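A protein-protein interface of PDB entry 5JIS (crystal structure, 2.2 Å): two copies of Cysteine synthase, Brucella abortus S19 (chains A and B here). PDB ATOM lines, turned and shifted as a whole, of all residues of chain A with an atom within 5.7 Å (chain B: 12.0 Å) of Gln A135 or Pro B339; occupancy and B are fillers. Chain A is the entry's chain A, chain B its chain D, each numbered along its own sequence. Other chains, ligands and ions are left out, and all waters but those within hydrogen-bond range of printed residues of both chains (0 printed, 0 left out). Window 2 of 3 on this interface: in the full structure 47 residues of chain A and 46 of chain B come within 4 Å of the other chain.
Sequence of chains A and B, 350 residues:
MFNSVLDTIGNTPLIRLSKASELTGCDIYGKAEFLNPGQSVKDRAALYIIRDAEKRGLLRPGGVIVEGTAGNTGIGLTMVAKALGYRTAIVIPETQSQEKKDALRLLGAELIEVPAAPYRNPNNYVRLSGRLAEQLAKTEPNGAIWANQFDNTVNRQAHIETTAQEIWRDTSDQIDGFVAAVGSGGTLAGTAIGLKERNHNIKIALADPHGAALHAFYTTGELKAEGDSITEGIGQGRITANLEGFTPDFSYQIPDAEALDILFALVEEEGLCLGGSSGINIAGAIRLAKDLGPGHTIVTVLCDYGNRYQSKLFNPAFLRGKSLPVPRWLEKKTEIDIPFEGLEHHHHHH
The side-chain amide oxygen (OD1) of Asn A123 is in hydrogen-bond range of the backbone NH (N) of Glu B341.
NH2 of Arg A131 is in hydrogen-bond range of O of Pro B339 (2.9 Å).
The side-chain amide oxygen of Gln A135 lies close to the backbone carbonyl oxygen of Asp B337 (2.9 Å).
Among the printed residues, merely in contact across the chains: Asn A123 with Phe B340, Leu A128 with Ile B338, Leu A128 with Pro B339, Leu A128 with Phe B340, Arg A131 with Glu B341, Leu A132 with Ile B336, Leu A132 with Pro B339 and Gln A135 with Pro B339.
No residue of chain B comes within 4 Å of Gly A130.
Of chain B, only Pro B339 and Glu B341 come within 4 Å of Arg A131.
Leu A132 touches just these residues of chain B: Ile B336 and Pro B339.
No residue of chain B comes within 4 Å of Ala A133.
Gln A135 touches just these residues of chain B: Asp B337 and Pro B339.
Leu A136 touches none of the printed residues of chain B.
No residue of chain B comes within 4 Å of Lys A138.
No residue of chain B comes within 4 Å of Thr A139.
Glu B335 touches none of the printed residues of chain A.
Of the printed residues of chain A, Ile B336 touches Leu A132.
Pro B339 touches just these residues of chain A: Leu A128 (3.2 Å), Arg A131 (2.9 Å), Leu A132 (3.8 Å) and Gln A135 (3.5 Å).
Of the printed residues of chain A, Glu B341 touches Asn A123 and Arg A131.
The nearest residue of chain B that does not touch Gln A135 is Ile B336 (4.1 Å).
Along chain B the printed residues that touch a printed residue of chain A span positions 336 to 341.
Of the 12 printed residues of chain A, 5 touch a printed residue of chain B.
Hydrophobic or aromatic side chains of chain A that line the printed part of chain B: Leu A128 and Leu A132.
No position is printed for both chains.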
ATOM      1  N   ASN A 123     -35.242 -16.335  19.730  1.00  0.00           N
ATOM      2  CA  ASN A 123     -34.358 -17.416  20.194  1.00  0.00           C
ATOM      3  C   ASN A 123     -33.488 -18.063  19.106  1.00  0.00           C
ATOM      4  O   ASN A 123     -32.787 -19.049  19.362  1.00  0.00           O
ATOM      5  CB  ASN A 123     -35.178 -18.473  20.922  1.00  0.00           C
ATOM      6  CG  ASN A 123     -35.852 -17.920  22.161  1.00  0.00           C
ATOM      7  OD1 ASN A 123     -35.359 -16.973  22.781  1.00  0.00           O
ATOM      8  ND2 ASN A 123     -36.981 -18.509  22.537  1.00  0.00           N
ATOM      9  N   LEU A 128     -29.968 -14.546  19.808  1.00  0.00           N
ATOM     10  CA  LEU A 128     -29.715 -14.988  21.181  1.00  0.00           C
ATOM     11  C   LEU A 128     -28.261 -14.736  21.629  1.00  0.00           C
ATOM     12  O   LEU A 128     -28.031 -14.329  22.772  1.00  0.00           O
ATOM     13  CB  LEU A 128     -30.057 -16.475  21.310  1.00  0.00           C
ATOM     14  CG  LEU A 128     -29.867 -17.162  22.669  1.00  0.00           C
ATOM     15  CD1 LEU A 128     -30.792 -16.575  23.726  1.00  0.00           C
ATOM     16  CD2 LEU A 128     -30.127 -18.652  22.534  1.00  0.00           C
ATOM     17  N   GLY A 130     -26.243 -12.402  20.600  1.00  0.00           N
ATOM     18  CA  GLY A 130     -26.169 -10.957  20.848  1.00  0.00           C
ATOM     19  C   GLY A 130     -26.622 -10.542  22.241  1.00  0.00           C
ATOM     20  O   GLY A 130     -25.962  -9.720  22.897  1.00  0.00           O
ATOM     21  N   ARG A 131     -27.732 -11.122  22.704  1.00  0.00           N
ATOM     22  CA  ARG A 131     -28.233 -10.829  24.049  1.00  0.00           C
ATOM     23  C   ARG A 131     -27.333 -11.433  25.133  1.00  0.00           C
ATOM     24  O   ARG A 131     -27.138 -10.824  26.196  1.00  0.00           O
ATOM     25  CB  ARG A 131     -29.694 -11.277  24.211  1.00  0.00           C
ATOM     26  CG  ARG A 131     -30.679 -10.488  23.340  1.00  0.00           C
ATOM     27  CD  ARG A 131     -32.123 -10.660  23.807  1.00  0.00           C
ATOM     28  NE  ARG A 131     -32.528 -12.071  23.878  1.00  0.00           N
ATOM     29  CZ  ARG A 131     -32.921 -12.830  22.846  1.00  0.00           C
ATOM     30  NH1 ARG A 131     -32.979 -12.348  21.603  1.00  0.00           N
ATOM     31  NH2 ARG A 131     -33.259 -14.105  23.059  1.00  0.00           N
ATOM     32  N   LEU A 132     -26.751 -12.598  24.856  1.00  0.00           N
ATOM     33  CA  LEU A 132     -25.766 -13.188  25.762  1.00  0.00           C
ATOM     34  C   LEU A 132     -24.521 -12.306  25.908  1.00  0.00           C
ATOM     35  O   LEU A 132     -24.036 -12.094  27.016  1.00  0.00           O
ATOM     36  CB  LEU A 132     -25.382 -14.595  25.292  1.00  0.00           C
ATOM     37  CG  LEU A 132     -24.353 -15.353  26.130  1.00  0.00           C
ATOM     38  CD1 LEU A 132     -24.828 -15.560  27.568  1.00  0.00           C
ATOM     39  CD2 LEU A 132     -24.037 -16.690  25.472  1.00  0.00           C
ATOM     40  N   ALA A 133     -24.005 -11.795  24.791  1.00  0.00           N
ATOM     41  CA  ALA A 133     -22.894 -10.819  24.822  1.00  0.00           C
ATOM     42  C   ALA A 133     -23.223  -9.588  25.679  1.00  0.00           C
ATOM     43  O   ALA A 133     -22.370  -9.098  26.433  1.00  0.00           O
ATOM     44  CB  ALA A 133     -22.510 -10.379  23.412  1.00  0.00           C
ATOM     45  N   GLU A 134     -24.449  -9.093  25.528  1.00  0.00           N
ATOM     46  CA  GLU A 134     -24.959  -7.956  26.314  1.00  0.00           C
ATOM     47  C   GLU A 134     -25.028  -8.301  27.807  1.00  0.00           C
ATOM     48  O   GLU A 134     -24.588  -7.528  28.651  1.00  0.00           O
ATOM     49  CB  GLU A 134     -26.344  -7.573  25.781  1.00  0.00           C
ATOM     50  CG  GLU A 134     -26.987  -6.314  26.341  1.00  0.00           C
ATOM     51  CD  GLU A 134     -28.305  -5.981  25.630  1.00  0.00           C
ATOM     52  OE1 GLU A 134     -28.676  -6.665  24.635  1.00  0.00           O
ATOM     53  OE2 GLU A 134     -28.982  -5.027  26.060  1.00  0.00           O
ATOM     54  N   GLN A 135     -25.561  -9.479  28.114  1.00  0.00           N
ATOM     55  CA  GLN A 135     -25.605  -9.987  29.488  1.00  0.00           C
ATOM     56  C   GLN A 135     -24.199 -10.137  30.109  1.00  0.00           C
ATOM     57  O   GLN A 135     -23.942  -9.640  31.208  1.00  0.00           O
ATOM     58  CB  GLN A 135     -26.356 -11.324  29.510  1.00  0.00           C
ATOM     59  CG  GLN A 135     -26.557 -11.935  30.888  1.00  0.00           C
ATOM     60  CD  GLN A 135     -27.184 -13.313  30.828  1.00  0.00           C
ATOM     61  OE1 GLN A 135     -26.593 -14.298  31.283  1.00  0.00           O
ATOM     62  NE2 GLN A 135     -28.376 -13.397  30.259  1.00  0.00           N
ATOM     63  N   LEU A 136     -23.295 -10.813  29.403  1.00  0.00           N
ATOM     64  CA  LEU A 136     -21.936 -11.054  29.912  1.00  0.00           C
ATOM     65  C   LEU A 136     -21.098  -9.793  30.060  1.00  0.00           C
ATOM     66  O   LEU A 136     -20.298  -9.683  30.999  1.00  0.00           O
ATOM     67  CB  LEU A 136     -21.190 -12.061  29.038  1.00  0.00           C
ATOM     68  CG  LEU A 136     -21.687 -13.502  29.104  1.00  0.00           C
ATOM     69  CD1 LEU A 136     -20.830 -14.346  28.181  1.00  0.00           C
ATOM     70  CD2 LEU A 136     -21.638 -14.052  30.523  1.00  0.00           C
ATOM     71  N   ALA A 137     -21.295  -8.843  29.145  1.00  0.00           N
ATOM     72  CA  ALA A 137     -20.655  -7.528  29.225  1.00  0.00           C
ATOM     73  C   ALA A 137     -20.829  -6.820  30.580  1.00  0.00           C
ATOM     74  O   ALA A 137     -19.927  -6.122  31.037  1.00  0.00           O
ATOM     75  CB  ALA A 137     -21.173  -6.643  28.103  1.00  0.00           C
ATOM     76  N   LYS A 138     -21.976  -7.015  31.224  1.00  0.00           N
ATOM     77  CA  LYS A 138     -22.246  -6.381  32.519  1.00  0.00           C
ATOM     78  C   LYS A 138     -21.346  -6.869  33.656  1.00  0.00           C
ATOM     79  O   LYS A 138     -21.109  -6.122  34.603  1.00  0.00           O
ATOM     80  CB  LYS A 138     -23.721  -6.546  32.902  1.00  0.00           C
ATOM     81  CG  LYS A 138     -24.639  -5.738  31.998  1.00  0.00           C
ATOM     82  CD  LYS A 138     -26.059  -5.654  32.547  1.00  0.00           C
ATOM     83  CE  LYS A 138     -26.850  -6.938  32.362  1.00  0.00           C
ATOM     84  NZ  LYS A 138     -28.254  -6.621  31.969  1.00  0.00           N
ATOM     85  N   THR A 139     -20.839  -8.101  33.555  1.00  0.00           N
ATOM     86  CA  THR A 139     -20.029  -8.699  34.611  1.00  0.00           C
ATOM     87  C   THR A 139     -18.706  -9.299  34.127  1.00  0.00           C
ATOM     88  O   THR A 139     -18.174 -10.223  34.764  1.00  0.00           O
ATOM     89  CB  THR A 139     -20.843  -9.787  35.322  1.00  0.00           C
ATOM     90  OG1 THR A 139     -21.119 -10.840  34.398  1.00  0.00           O
ATOM     91  CG2 THR A 139     -22.171  -9.208  35.872  1.00  0.00           C
ATOM     92  N   GLU B 335     -23.618 -24.190  31.916  1.00  0.00           N
ATOM     93  CA  GLU B 335     -23.200 -23.403  33.076  1.00  0.00           C
ATOM     94  C   GLU B 335     -23.927 -22.043  33.156  1.00  0.00           C
ATOM     95  O   GLU B 335     -24.575 -21.744  34.162  1.00  0.00           O
ATOM     96  CB  GLU B 335     -21.677 -23.204  33.047  1.00  0.00           C
ATOM     97  CG  GLU B 335     -21.040 -22.887  34.399  1.00  0.00           C
ATOM     98  CD  GLU B 335     -20.738 -24.117  35.258  1.00  0.00           C
ATOM     99  OE1 GLU B 335     -20.228 -25.128  34.717  1.00  0.00           O
ATOM    100  OE2 GLU B 335     -20.985 -24.062  36.488  1.00  0.00           O
ATOM    101  N   ILE B 336     -23.827 -21.241  32.095  1.00  0.00           N
ATOM    102  CA  ILE B 336     -24.360 -19.859  32.075  1.00  0.00           C
ATOM    103  C   ILE B 336     -25.894 -19.821  31.934  1.00  0.00           C
ATOM    104  O   ILE B 336     -26.496 -20.728  31.359  1.00  0.00           O
ATOM    105  CB  ILE B 336     -23.692 -19.030  30.935  1.00  0.00           C
ATOM    106  CG1 ILE B 336     -22.190 -18.879  31.198  1.00  0.00           C
ATOM    107  CG2 ILE B 336     -24.308 -17.632  30.796  1.00  0.00           C
ATOM    108  CD1 ILE B 336     -21.378 -18.456  29.990  1.00  0.00           C
ATOM    109  N   ASP B 337     -26.508 -18.762  32.468  1.00  0.00           N
ATOM    110  CA  ASP B 337     -27.939 -18.486  32.278  1.00  0.00           C
ATOM    111  C   ASP B 337     -28.203 -17.922  30.860  1.00  0.00           C
ATOM    112  O   ASP B 337     -27.792 -16.806  30.537  1.00  0.00           O
ATOM    113  CB  ASP B 337     -28.433 -17.506  33.356  1.00  0.00           C
ATOM    114  CG  ASP B 337     -29.925 -17.613  33.612  1.00  0.00           C
ATOM    115  OD1 ASP B 337     -30.719 -17.597  32.645  1.00  0.00           O
ATOM    116  OD2 ASP B 337     -30.307 -17.715  34.797  1.00  0.00           O
ATOM    117  N   ILE B 338     -28.922 -18.682  30.037  1.00  0.00           N
ATOM    118  CA  ILE B 338     -29.119 -18.344  28.625  1.00  0.00           C
ATOM    119  C   ILE B 338     -30.361 -17.442  28.511  1.00  0.00           C
ATOM    120  O   ILE B 338     -31.430 -17.828  28.975  1.00  0.00           O
ATOM    121  CB  ILE B 338     -29.307 -19.612  27.758  1.00  0.00           C
ATOM    122  CG1 ILE B 338     -28.332 -20.743  28.149  1.00  0.00           C
ATOM    123  CG2 ILE B 338     -29.145 -19.278  26.282  1.00  0.00           C
ATOM    124  CD1 ILE B 338     -26.867 -20.351  28.211  1.00  0.00           C
ATOM    125  N   PRO B 339     -30.240 -16.247  27.891  1.00  0.00           N
ATOM    126  CA  PRO B 339     -31.390 -15.330  27.843  1.00  0.00           C
ATOM    127  C   PRO B 339     -32.410 -15.624  26.722  1.00  0.00           C
ATOM    128  O   PRO B 339     -32.551 -14.854  25.776  1.00  0.00           O
ATOM    129  CB  PRO B 339     -30.726 -13.960  27.679  1.00  0.00           C
ATOM    130  CG  PRO B 339     -29.486 -14.249  26.904  1.00  0.00           C
ATOM    131  CD  PRO B 339     -29.049 -15.648  27.259  1.00  0.00           C
ATOM    132  N   PHE B 340     -33.123 -16.739  26.852  1.00  0.00           N
ATOM    133  CA  PHE B 340     -34.249 -17.061  25.972  1.00  0.00           C
ATOM    134  C   PHE B 340     -35.370 -16.042  26.194  1.00  0.00           C
ATOM    135  O   PHE B 340     -35.577 -15.587  27.323  1.00  0.00           O
ATOM    136  CB  PHE B 340     -34.765 -18.477  26.242  1.00  0.00           C
ATOM    137  CG  PHE B 340     -33.856 -19.564  25.742  1.00  0.00           C
ATOM    138  CD1 PHE B 340     -33.809 -19.880  24.384  1.00  0.00           C
ATOM    139  CD2 PHE B 340     -33.063 -20.293  26.621  1.00  0.00           C
ATOM    140  CE1 PHE B 340     -32.980 -20.886  23.908  1.00  0.00           C
ATOM    141  CE2 PHE B 340     -32.232 -21.309  26.154  1.00  0.00           C
ATOM    142  CZ  PHE B 340     -32.186 -21.603  24.795  1.00  0.00           C
ATOM    143  N   GLU B 341     -36.053 -15.688  25.104  1.00  0.00           N
ATOM    144  CA  GLU B 341     -37.113 -14.662  25.055  1.00  0.00           C
ATOM    145  C   GLU B 341     -36.630 -13.258  25.431  1.00  0.00           C
ATOM    146  O   GLU B 341     -36.515 -12.379  24.567  1.00  0.00           O
ATOM    147  CB  GLU B 341     -38.324 -15.064  25.903  1.00  0.00           C
ATOM    148  CG  GLU B 341     -38.900 -16.424  25.547  1.00  0.00           C
ATOM    149  CD  GLU B 341     -40.238 -16.680  26.221  1.00  0.00           C
ATOM    150  OE1 GLU B 341     -41.164 -15.871  26.008  1.00  0.00           O
ATOM    151  OE2 GLU B 341     -40.372 -17.690  26.955  1.00  0.00           O
